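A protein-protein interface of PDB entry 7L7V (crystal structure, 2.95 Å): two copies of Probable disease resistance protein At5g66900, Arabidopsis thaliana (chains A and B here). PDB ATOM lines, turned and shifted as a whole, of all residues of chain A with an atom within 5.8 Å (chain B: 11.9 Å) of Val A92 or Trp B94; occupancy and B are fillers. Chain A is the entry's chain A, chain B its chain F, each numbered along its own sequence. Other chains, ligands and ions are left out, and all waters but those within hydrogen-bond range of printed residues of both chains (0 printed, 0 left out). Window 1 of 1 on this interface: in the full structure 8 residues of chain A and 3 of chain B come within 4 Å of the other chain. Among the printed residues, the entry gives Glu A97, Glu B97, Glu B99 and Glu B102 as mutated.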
ATOM      1  N   PHE A  37     -31.348   5.327 -11.772  1.00  0.00           N
ATOM      2  CA  PHE A  37     -30.123   4.567 -12.104  1.00  0.00           C
ATOM      3  C   PHE A  37     -30.219   4.110 -13.545  1.00  0.00           C
ATOM      4  O   PHE A  37     -30.663   3.033 -13.760  1.00  0.00           O
ATOM      5  CB  PHE A  37     -29.876   3.387 -11.178  1.00  0.00           C
ATOM      6  CG  PHE A  37     -28.500   2.796 -11.369  1.00  0.00           C
ATOM      7  CD1 PHE A  37     -27.350   3.542 -11.185  1.00  0.00           C
ATOM      8  CD2 PHE A  37     -28.353   1.473 -11.696  1.00  0.00           C
ATOM      9  CE1 PHE A  37     -26.092   3.004 -11.351  1.00  0.00           C
ATOM     10  CE2 PHE A  37     -27.091   0.913 -11.815  1.00  0.00           C
ATOM     11  CZ  PHE A  37     -25.969   1.696 -11.696  1.00  0.00           C
ATOM     12  N   LYS A  88     -30.998  -7.182  -6.329  1.00  0.00           N
ATOM     13  CA  LYS A  88     -29.801  -7.051  -5.467  1.00  0.00           C
ATOM     14  C   LYS A  88     -29.398  -5.593  -5.352  1.00  0.00           C
ATOM     15  O   LYS A  88     -28.503  -5.316  -4.537  1.00  0.00           O
ATOM     16  CB  LYS A  88     -28.654  -7.810  -6.106  1.00  0.00           C
ATOM     17  CG  LYS A  88     -27.425  -7.970  -5.256  1.00  0.00           C
ATOM     18  CD  LYS A  88     -26.124  -7.648  -5.943  1.00  0.00           C
ATOM     19  CE  LYS A  88     -25.863  -8.620  -7.050  1.00  0.00           C
ATOM     20  NZ  LYS A  88     -24.510  -8.393  -7.586  1.00  0.00           N
ATOM     21  N   PHE A  89     -30.012  -4.705  -6.140  1.00  0.00           N
ATOM     22  CA  PHE A  89     -29.563  -3.304  -6.296  1.00  0.00           C
ATOM     23  C   PHE A  89     -29.724  -2.526  -4.995  1.00  0.00           C
ATOM     24  O   PHE A  89     -28.853  -1.734  -4.610  1.00  0.00           O
ATOM     25  CB  PHE A  89     -30.327  -2.620  -7.411  1.00  0.00           C
ATOM     26  CG  PHE A  89     -29.793  -1.265  -7.742  1.00  0.00           C
ATOM     27  CD1 PHE A  89     -28.487  -1.109  -8.203  1.00  0.00           C
ATOM     28  CD2 PHE A  89     -30.608  -0.170  -7.626  1.00  0.00           C
ATOM     29  CE1 PHE A  89     -27.983   0.150  -8.497  1.00  0.00           C
ATOM     30  CE2 PHE A  89     -30.099   1.079  -7.931  1.00  0.00           C
ATOM     31  CZ  PHE A  89     -28.792   1.242  -8.346  1.00  0.00           C
ATOM     32  N   PRO A  90     -30.828  -2.703  -4.248  1.00  0.00           N
ATOM     33  CA  PRO A  90     -30.945  -2.041  -2.952  1.00  0.00           C
ATOM     34  C   PRO A  90     -29.784  -2.291  -1.978  1.00  0.00           C
ATOM     35  O   PRO A  90     -29.740  -1.682  -1.001  1.00  0.00           O
ATOM     36  CB  PRO A  90     -32.229  -2.667  -2.372  1.00  0.00           C
ATOM     37  CG  PRO A  90     -33.039  -3.016  -3.581  1.00  0.00           C
ATOM     38  CD  PRO A  90     -32.019  -3.487  -4.594  1.00  0.00           C
ATOM     39  N   ARG A  91     -28.890  -3.216  -2.239  1.00  0.00           N
ATOM     40  CA  ARG A  91     -27.822  -3.562  -1.279  1.00  0.00           C
ATOM     41  C   ARG A  91     -26.460  -3.144  -1.878  1.00  0.00           C
ATOM     42  O   ARG A  91     -25.436  -3.237  -1.165  1.00  0.00           O
ATOM     43  CB  ARG A  91     -27.901  -5.060  -0.913  1.00  0.00           C
ATOM     44  N   VAL A  92     -26.387  -2.714  -3.144  1.00  0.00           N
ATOM     45  CA  VAL A  92     -25.092  -2.177  -3.640  1.00  0.00           C
ATOM     46  C   VAL A  92     -24.879  -0.817  -2.982  1.00  0.00           C
ATOM     47  O   VAL A  92     -25.824  -0.046  -2.872  1.00  0.00           O
ATOM     48  CB  VAL A  92     -24.992  -2.169  -5.173  1.00  0.00           C
ATOM     49  CG1 VAL A  92     -25.686  -3.371  -5.748  1.00  0.00           C
ATOM     50  CG2 VAL A  92     -25.613  -0.970  -5.765  1.00  0.00           C
ATOM     51  N   LYS A  93     -23.647  -0.555  -2.573  1.00  0.00           N
ATOM     52  CA  LYS A  93     -23.297   0.689  -1.855  1.00  0.00           C
ATOM     53  C   LYS A  93     -22.635   1.647  -2.844  1.00  0.00           C
ATOM     54  O   LYS A  93     -22.277   1.205  -3.942  1.00  0.00           O
ATOM     55  CB  LYS A  93     -22.383   0.334  -0.688  1.00  0.00           C
ATOM     56  CG  LYS A  93     -22.770  -0.932   0.073  1.00  0.00           C
ATOM     57  CD  LYS A  93     -21.895  -1.306   1.218  1.00  0.00           C
ATOM     58  CE  LYS A  93     -22.136  -0.381   2.398  1.00  0.00           C
ATOM     59  NZ  LYS A  93     -21.125  -0.400   3.506  1.00  0.00           N
ATOM     60  N   TRP A  94     -22.480   2.916  -2.477  1.00  0.00           N
ATOM     61  CA  TRP A  94     -22.009   3.946  -3.460  1.00  0.00           C
ATOM     62  C   TRP A  94     -20.617   3.587  -4.002  1.00  0.00           C
ATOM     63  O   TRP A  94     -20.292   3.999  -5.135  1.00  0.00           O
ATOM     64  CB  TRP A  94     -21.954   5.336  -2.853  1.00  0.00           C
ATOM     65  CG  TRP A  94     -20.992   5.446  -1.725  1.00  0.00           C
ATOM     66  CD1 TRP A  94     -21.277   5.311  -0.403  1.00  0.00           C
ATOM     67  CD2 TRP A  94     -19.591   5.737  -1.813  1.00  0.00           C
ATOM     68  NE1 TRP A  94     -20.144   5.474   0.343  1.00  0.00           N
ATOM     69  CE2 TRP A  94     -19.095   5.743  -0.485  1.00  0.00           C
ATOM     70  CE3 TRP A  94     -18.710   5.979  -2.871  1.00  0.00           C
ATOM     71  CZ2 TRP A  94     -17.759   6.001  -0.190  1.00  0.00           C
ATOM     72  CZ3 TRP A  94     -17.398   6.252  -2.586  1.00  0.00           C
ATOM     73  CH2 TRP A  94     -16.938   6.284  -1.259  1.00  0.00           C
ATOM     74  N   GLU A  96     -19.555   0.706  -4.731  1.00  0.00           N
ATOM     75  CA  GLU A  96     -19.666  -0.455  -5.661  1.00  0.00           C
ATOM     76  C   GLU A  96     -20.291  -0.052  -7.013  1.00  0.00           C
ATOM     77  O   GLU A  96     -20.485  -0.927  -7.813  1.00  0.00           O
ATOM     78  CB  GLU A  96     -20.487  -1.575  -5.004  1.00  0.00           C
ATOM     79  CG  GLU A  96     -20.137  -1.779  -3.559  1.00  0.00           C
ATOM     80  CD  GLU A  96     -20.528  -3.104  -2.972  1.00  0.00           C
ATOM     81  OE1 GLU A  96     -19.646  -3.940  -2.957  1.00  0.00           O
ATOM     82  OE2 GLU A  96     -21.670  -3.274  -2.475  1.00  0.00           O
ATOM     83  N   GLU A  97     -20.647   1.195  -7.279  1.00  0.00           N
ATOM     84  CA  GLU A  97     -21.422   1.513  -8.507  1.00  0.00           C
ATOM     85  C   GLU A  97     -20.729   0.849  -9.683  1.00  0.00           C
ATOM     86  O   GLU A  97     -21.386   0.160 -10.420  1.00  0.00           O
ATOM     87  CB  GLU A  97     -21.547   3.025  -8.709  1.00  0.00           C
ATOM     88  CG  GLU A  97     -22.145   3.529 -10.015  1.00  0.00           C
ATOM     89  CD  GLU A  97     -22.276   5.066 -10.039  1.00  0.00           C
ATOM     90  OE1 GLU A  97     -22.884   5.681 -10.982  1.00  0.00           O
ATOM     91  OE2 GLU A  97     -21.804   5.692  -9.084  1.00  0.00           O
ATOM     92  N   TYR A 100     -21.108  -3.050 -10.000  1.00  0.00           N
ATOM     93  CA  TYR A 100     -22.488  -3.439 -10.318  1.00  0.00           C
ATOM     94  C   TYR A 100     -22.760  -3.067 -11.765  1.00  0.00           C
ATOM     95  O   TYR A 100     -23.445  -3.823 -12.467  1.00  0.00           O
ATOM     96  CB  TYR A 100     -23.490  -2.763  -9.393  1.00  0.00           C
ATOM     97  CG  TYR A 100     -24.913  -3.210  -9.638  1.00  0.00           C
ATOM     98  CD1 TYR A 100     -25.380  -4.436  -9.179  1.00  0.00           C
ATOM     99  CD2 TYR A 100     -25.790  -2.395 -10.328  1.00  0.00           C
ATOM    100  CE1 TYR A 100     -26.673  -4.837  -9.421  1.00  0.00           C
ATOM    101  CE2 TYR A 100     -27.102  -2.765 -10.538  1.00  0.00           C
ATOM    102  CZ  TYR A 100     -27.545  -3.981 -10.067  1.00  0.00           C
ATOM    103  OH  TYR A 100     -28.838  -4.347 -10.327  1.00  0.00           O
ATOM    104  N   PHE B  37     -21.907  18.410   0.572  1.00  0.00           N
ATOM    105  CA  PHE B  37     -22.728  18.555  -0.653  1.00  0.00           C
ATOM    106  C   PHE B  37     -22.739  20.039  -1.008  1.00  0.00           C
ATOM    107  O   PHE B  37     -23.401  20.839  -0.359  1.00  0.00           O
ATOM    108  CB  PHE B  37     -24.118  17.942  -0.506  1.00  0.00           C
ATOM    109  CG  PHE B  37     -24.801  17.666  -1.812  1.00  0.00           C
ATOM    110  CD1 PHE B  37     -24.253  16.785  -2.696  1.00  0.00           C
ATOM    111  CD2 PHE B  37     -25.991  18.276  -2.153  1.00  0.00           C
ATOM    112  CE1 PHE B  37     -24.844  16.532  -3.923  1.00  0.00           C
ATOM    113  CE2 PHE B  37     -26.615  17.981  -3.355  1.00  0.00           C
ATOM    114  CZ  PHE B  37     -26.036  17.109  -4.250  1.00  0.00           C
ATOM    115  N   LYS B  88     -35.162  16.324   3.099  1.00  0.00           N
ATOM    116  CA  LYS B  88     -35.094  14.916   2.641  1.00  0.00           C
ATOM    117  C   LYS B  88     -33.702  14.528   2.147  1.00  0.00           C
ATOM    118  O   LYS B  88     -33.497  13.391   1.766  1.00  0.00           O
ATOM    119  CB  LYS B  88     -36.091  14.701   1.514  1.00  0.00           C
ATOM    120  CG  LYS B  88     -35.727  15.351   0.199  1.00  0.00           C
ATOM    121  CD  LYS B  88     -36.259  14.512  -0.961  1.00  0.00           C
ATOM    122  CE  LYS B  88     -36.740  15.319  -2.157  1.00  0.00           C
ATOM    123  NZ  LYS B  88     -36.716  14.522  -3.400  1.00  0.00           N
ATOM    124  N   PHE B  89     -32.740  15.420   2.181  1.00  0.00           N
ATOM    125  CA  PHE B  89     -31.388  15.127   1.661  1.00  0.00           C
ATOM    126  C   PHE B  89     -30.810  13.896   2.358  1.00  0.00           C
ATOM    127  O   PHE B  89     -30.154  13.074   1.722  1.00  0.00           O
ATOM    128  CB  PHE B  89     -30.460  16.331   1.751  1.00  0.00           C
ATOM    129  CG  PHE B  89     -29.099  16.031   1.178  1.00  0.00           C
ATOM    130  CD1 PHE B  89     -28.935  15.743  -0.173  1.00  0.00           C
ATOM    131  CD2 PHE B  89     -27.983  16.046   1.998  1.00  0.00           C
ATOM    132  CE1 PHE B  89     -27.670  15.510  -0.688  1.00  0.00           C
ATOM    133  CE2 PHE B  89     -26.729  15.769   1.488  1.00  0.00           C
ATOM    134  CZ  PHE B  89     -26.579  15.503   0.147  1.00  0.00           C
ATOM    135  N   PRO B  90     -30.950  13.733   3.691  1.00  0.00           N
ATOM    136  CA  PRO B  90     -30.487  12.507   4.349  1.00  0.00           C
ATOM    137  C   PRO B  90     -30.987  11.203   3.699  1.00  0.00           C
ATOM    138  O   PRO B  90     -30.333  10.206   3.820  1.00  0.00           O
ATOM    139  CB  PRO B  90     -31.081  12.638   5.746  1.00  0.00           C
ATOM    140  CG  PRO B  90     -31.036  14.105   5.944  1.00  0.00           C
ATOM    141  CD  PRO B  90     -31.504  14.697   4.643  1.00  0.00           C
ATOM    142  N   ARG B  91     -32.164  11.222   3.082  1.00  0.00           N
ATOM    143  CA  ARG B  91     -32.800  10.008   2.507  1.00  0.00           C
ATOM    144  C   ARG B  91     -32.472   9.871   1.015  1.00  0.00           C
ATOM    145  O   ARG B  91     -33.066   9.016   0.371  1.00  0.00           O
ATOM    146  CB  ARG B  91     -34.310  10.075   2.635  1.00  0.00           C
ATOM    147  CG  ARG B  91     -34.799   9.901   4.047  1.00  0.00           C
ATOM    148  CD  ARG B  91     -36.315   9.684   4.046  1.00  0.00           C
ATOM    149  NE  ARG B  91     -36.909  10.180   2.809  1.00  0.00           N
ATOM    150  CZ  ARG B  91     -37.612  11.312   2.612  1.00  0.00           C
ATOM    151  NH1 ARG B  91     -37.872  12.152   3.611  1.00  0.00           N
ATOM    152  NH2 ARG B  91     -38.048  11.571   1.382  1.00  0.00           N
ATOM    153  N   VAL B  92     -31.604  10.708   0.499  1.00  0.00           N
ATOM    154  CA  VAL B  92     -31.339  10.719  -0.949  1.00  0.00           C
ATOM    155  C   VAL B  92     -30.261   9.691  -1.232  1.00  0.00           C
ATOM    156  O   VAL B  92     -29.183   9.736  -0.599  1.00  0.00           O
ATOM    157  CB  VAL B  92     -30.931  12.095  -1.499  1.00  0.00           C
ATOM    158  CG1 VAL B  92     -30.655  12.024  -2.959  1.00  0.00           C
ATOM    159  CG2 VAL B  92     -32.025  13.109  -1.256  1.00  0.00           C
ATOM    160  N   LYS B  93     -30.500   8.871  -2.244  1.00  0.00           N
ATOM    161  CA  LYS B  93     -29.648   7.685  -2.473  1.00  0.00           C
ATOM    162  C   LYS B  93     -28.539   7.993  -3.486  1.00  0.00           C
ATOM    163  O   LYS B  93     -28.707   8.879  -4.318  1.00  0.00           O
ATOM    164  CB  LYS B  93     -30.579   6.507  -2.747  1.00  0.00           C
ATOM    165  CG  LYS B  93     -31.294   6.048  -1.477  1.00  0.00           C
ATOM    166  CD  LYS B  93     -32.283   4.935  -1.636  1.00  0.00           C
ATOM    167  CE  LYS B  93     -33.615   5.227  -0.957  1.00  0.00           C
ATOM    168  NZ  LYS B  93     -34.459   6.190  -1.750  1.00  0.00           N
ATOM    169  N   TRP B  94     -27.422   7.275  -3.408  1.00  0.00           N
ATOM    170  CA  TRP B  94     -26.264   7.617  -4.274  1.00  0.00           C
ATOM    171  C   TRP B  94     -26.711   7.671  -5.739  1.00  0.00           C
ATOM    172  O   TRP B  94     -26.154   8.447  -6.483  1.00  0.00           O
ATOM    173  CB  TRP B  94     -25.082   6.658  -4.061  1.00  0.00           C
ATOM    174  CG  TRP B  94     -25.336   5.218  -4.404  1.00  0.00           C
ATOM    175  CD1 TRP B  94     -25.721   4.252  -3.534  1.00  0.00           C
ATOM    176  CD2 TRP B  94     -25.248   4.581  -5.693  1.00  0.00           C
ATOM    177  NE1 TRP B  94     -25.800   3.038  -4.167  1.00  0.00           N
ATOM    178  CE2 TRP B  94     -25.534   3.223  -5.496  1.00  0.00           C
ATOM    179  CE3 TRP B  94     -24.922   5.014  -6.976  1.00  0.00           C
ATOM    180  CZ2 TRP B  94     -25.564   2.325  -6.555  1.00  0.00           C
ATOM    181  CZ3 TRP B  94     -24.947   4.131  -8.023  1.00  0.00           C
ATOM    182  CH2 TRP B  94     -25.263   2.796  -7.810  1.00  0.00           C
ATOM    183  N   TYR B  95     -27.667   6.868  -6.130  1.00  0.00           N
ATOM    184  CA  TYR B  95     -28.121   6.823  -7.516  1.00  0.00           C
ATOM    185  C   TYR B  95     -29.019   7.993  -7.797  1.00  0.00           C
ATOM    186  O   TYR B  95     -29.235   8.263  -8.994  1.00  0.00           O
ATOM    187  CB  TYR B  95     -28.771   5.489  -7.874  1.00  0.00           C
ATOM    188  CG  TYR B  95     -29.915   4.978  -7.046  1.00  0.00           C
ATOM    189  CD1 TYR B  95     -31.211   5.197  -7.460  1.00  0.00           C
ATOM    190  CD2 TYR B  95     -29.689   4.223  -5.909  1.00  0.00           C
ATOM    191  CE1 TYR B  95     -32.280   4.693  -6.755  1.00  0.00           C
ATOM    192  CE2 TYR B  95     -30.742   3.713  -5.189  1.00  0.00           C
ATOM    193  CZ  TYR B  95     -32.039   3.944  -5.622  1.00  0.00           C
ATOM    194  OH  TYR B  95     -33.104   3.420  -4.940  1.00  0.00           O
ATOM    195  N   GLU B  96     -29.441   8.726  -6.787  1.00  0.00           N
ATOM    196  CA  GLU B  96     -30.362   9.875  -7.034  1.00  0.00           C
ATOM    197  C   GLU B  96     -29.572  11.193  -7.018  1.00  0.00           C
ATOM    198  O   GLU B  96     -30.199  12.232  -7.122  1.00  0.00           O
ATOM    199  CB  GLU B  96     -31.557   9.867  -6.093  1.00  0.00           C
ATOM    200  CG  GLU B  96     -32.196   8.505  -5.923  1.00  0.00           C
ATOM    201  CD  GLU B  96     -33.211   8.383  -4.782  1.00  0.00           C
ATOM    202  OE1 GLU B  96     -33.135   9.138  -3.790  1.00  0.00           O
ATOM    203  OE2 GLU B  96     -34.030   7.480  -4.850  1.00  0.00           O
ATOM    204  N   GLU B  97     -28.245  11.163  -6.911  1.00  0.00           N
ATOM    205  CA  GLU B  97     -27.435  12.394  -6.859  1.00  0.00           C
ATOM    206  C   GLU B  97     -27.803  13.328  -8.019  1.00  0.00           C
ATOM    207  O   GLU B  97     -28.171  14.457  -7.785  1.00  0.00           O
ATOM    208  CB  GLU B  97     -25.945  12.090  -6.858  1.00  0.00           C
ATOM    209  CG  GLU B  97     -25.071  13.327  -7.073  1.00  0.00           C
ATOM    210  CD  GLU B  97     -23.579  13.143  -6.787  1.00  0.00           C
ATOM    211  OE1 GLU B  97     -22.926  14.096  -6.424  1.00  0.00           O
ATOM    212  OE2 GLU B  97     -23.050  12.035  -6.929  1.00  0.00           O
ATOM    213  N   SER B  98     -27.696  12.879  -9.246  1.00  0.00           N
ATOM    214  CA  SER B  98     -27.922  13.761 -10.425  1.00  0.00           C
ATOM    215  C   SER B  98     -29.375  14.230 -10.407  1.00  0.00           C
ATOM    216  O   SER B  98     -29.577  15.431 -10.473  1.00  0.00           O
ATOM    217  CB  SER B  98     -27.599  13.047 -11.686  1.00  0.00           C
ATOM    218  OG  SER B  98     -27.996  11.705 -11.457  1.00  0.00           O
ATOM    219  N   GLU B  99     -30.338  13.315 -10.304  1.00  0.00           N
ATOM    220  CA  GLU B  99     -31.764  13.707 -10.221  1.00  0.00           C
ATOM    221  C   GLU B  99     -31.904  14.806  -9.161  1.00  0.00           C
ATOM    222  O   GLU B  99     -32.544  15.829  -9.420  1.00  0.00           O
ATOM    223  CB  GLU B  99     -32.608  12.507  -9.823  1.00  0.00           C
ATOM    224  CG  GLU B  99     -33.718  12.141 -10.782  1.00  0.00           C
ATOM    225  CD  GLU B  99     -34.640  11.093 -10.173  1.00  0.00           C
ATOM    226  OE1 GLU B  99     -34.719  11.016  -8.932  1.00  0.00           O
ATOM    227  OE2 GLU B  99     -35.245  10.314 -10.946  1.00  0.00           O
ATOM    228  N   TYR B 100     -31.393  14.565  -7.958  1.00  0.00           N
ATOM    229  CA  TYR B 100     -31.598  15.489  -6.825  1.00  0.00           C
ATOM    230  C   TYR B 100     -30.884  16.790  -7.133  1.00  0.00           C
ATOM    231  O   TYR B 100     -31.468  17.833  -6.830  1.00  0.00           O
ATOM    232  CB  TYR B 100     -31.040  14.924  -5.541  1.00  0.00           C
ATOM    233  CG  TYR B 100     -31.226  15.812  -4.340  1.00  0.00           C
ATOM    234  CD1 TYR B 100     -32.412  15.861  -3.642  1.00  0.00           C
ATOM    235  CD2 TYR B 100     -30.181  16.565  -3.865  1.00  0.00           C
ATOM    236  CE1 TYR B 100     -32.561  16.626  -2.510  1.00  0.00           C
ATOM    237  CE2 TYR B 100     -30.310  17.333  -2.721  1.00  0.00           C
ATOM    238  CZ  TYR B 100     -31.508  17.372  -2.040  1.00  0.00           C
ATOM    239  OH  TYR B 100     -31.659  18.173  -0.942  1.00  0.00           O
ATOM    240  N   THR B 101     -29.698  16.740  -7.749  1.00  0.00           N
ATOM    241  CA  THR B 101     -28.905  17.960  -8.071  1.00  0.00           C
ATOM    242  C   THR B 101     -29.711  18.845  -9.027  1.00  0.00           C
ATOM    243  O   THR B 101     -29.706  20.070  -8.834  1.00  0.00           O
ATOM    244  CB  THR B 101     -27.486  17.632  -8.561  1.00  0.00           C
ATOM    245  OG1 THR B 101     -26.841  16.838  -7.559  1.00  0.00           O
ATOM    246  CG2 THR B 101     -26.675  18.886  -8.841  1.00  0.00           C
ATOM    247  N   GLU B 102     -30.368  18.262 -10.023  1.00  0.00           N
ATOM    248  CA  GLU B 102     -31.186  19.047 -10.982  1.00  0.00           C
ATOM    249  C   GLU B 102     -32.261  19.780 -10.207  1.00  0.00           C
ATOM    250  O   GLU B 102     -32.436  20.978 -10.424  1.00  0.00           O
ATOM    251  CB  GLU B 102     -31.872  18.148 -11.995  1.00  0.00           C
ATOM    252  CG  GLU B 102     -30.900  17.372 -12.877  1.00  0.00           C
ATOM    253  CD  GLU B 102     -31.622  16.441 -13.832  1.00  0.00           C
ATOM    254  OE1 GLU B 102     -32.782  16.835 -14.246  1.00  0.00           O
ATOM    255  OE2 GLU B 102     -31.030  15.406 -14.293  1.00  0.00           O
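O of Val A92 lies within hydrogen-bond range of NE1 of Trp B94, at 3.3 Å.
The side-chain carboxylate (OE2) of Glu A96 lies within hydrogen-bond range of the backbone NH (N) of Lys A93 (3.4 Å).
Among the printed residues, merely in contact across the chains: Phe A37 with Trp B94 (3.6 Å), Phe A89 with Trp B94 (3.8 Å), Phe A89 with Tyr B95 (3.8 Å), Lys A93 with Trp B94 (3.7 Å), Trp A94 with Trp B94 (3.6 Å) and Glu A97 with Trp B94 (3.5 Å).
Of chain B, only Trp B94 (3.3 Å) comes within 4 Å of Val A92.
Trp B94 touches just these residues of chain A: Phe A37 (3.6 Å), Phe A89 (3.8 Å), Val A92 (3.3 Å), Lys A93 (3.7 Å), Trp A94 (3.6 Å) and Glu A97 (3.5 Å).
No residue of chain B comes within 4 Å of Lys A88.
Phe A89 touches two residues of chain B.
No residue of chain B comes within 4 Å of Pro A90.
Of chain B, only Trp B94 (3.7 Å) comes within 4 Å of Lys A93.
No residue of chain B comes within 4 Å of Glu A96.
Glu A97 touches just one residue of chain B: Trp B94 (3.5 Å).
No residue of chain B comes within 4 Å of Tyr A100.
Of the printed residues of chain B, Trp A94 touches Trp B94 (3.6 Å).
Of the printed residues of chain B, Phe A37 touches Trp B94 (3.6 Å).
The nearest printed residue of chain A that does not touch Trp B94 is Glu A96 (5.8 Å).
The nearest printed residue of chain B that does not touch Phe A37 is Tyr B95 (4.1 Å).
Hydrophobic or aromatic side chains of chain A within 4 Å of the printed part of chain B: Phe A37, Phe A89, Val A92 and Trp A94.
Among the printed residues, 7 pairs touch across the chains.
Among the printed residues, no Asp or Glu carboxylate lies within 4 Å of a Lys or Arg side-chain nitrogen of the other chain.
Phe A37 touches Trp B94, but with the chains exchanged Trp A94 does not touch Phe B37 (11.6 Å).
Phe A89 touches Trp B94, but with the chains exchanged Trp A94 does not touch Phe B89 (11.5 Å).
Lys A93 touches Trp B94, but with the chains exchanged Trp A94 does not touch Lys B93 (7.1 Å).
Glu A97 touches Trp B94, but with the chains exchanged Trp A94 does not touch Glu B97 (7.9 Å).
11 positions are printed for both chains.
Of the 7 pairs that touch across the chains among the printed residues, 1 has its exchanged pair printed and touching as well.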
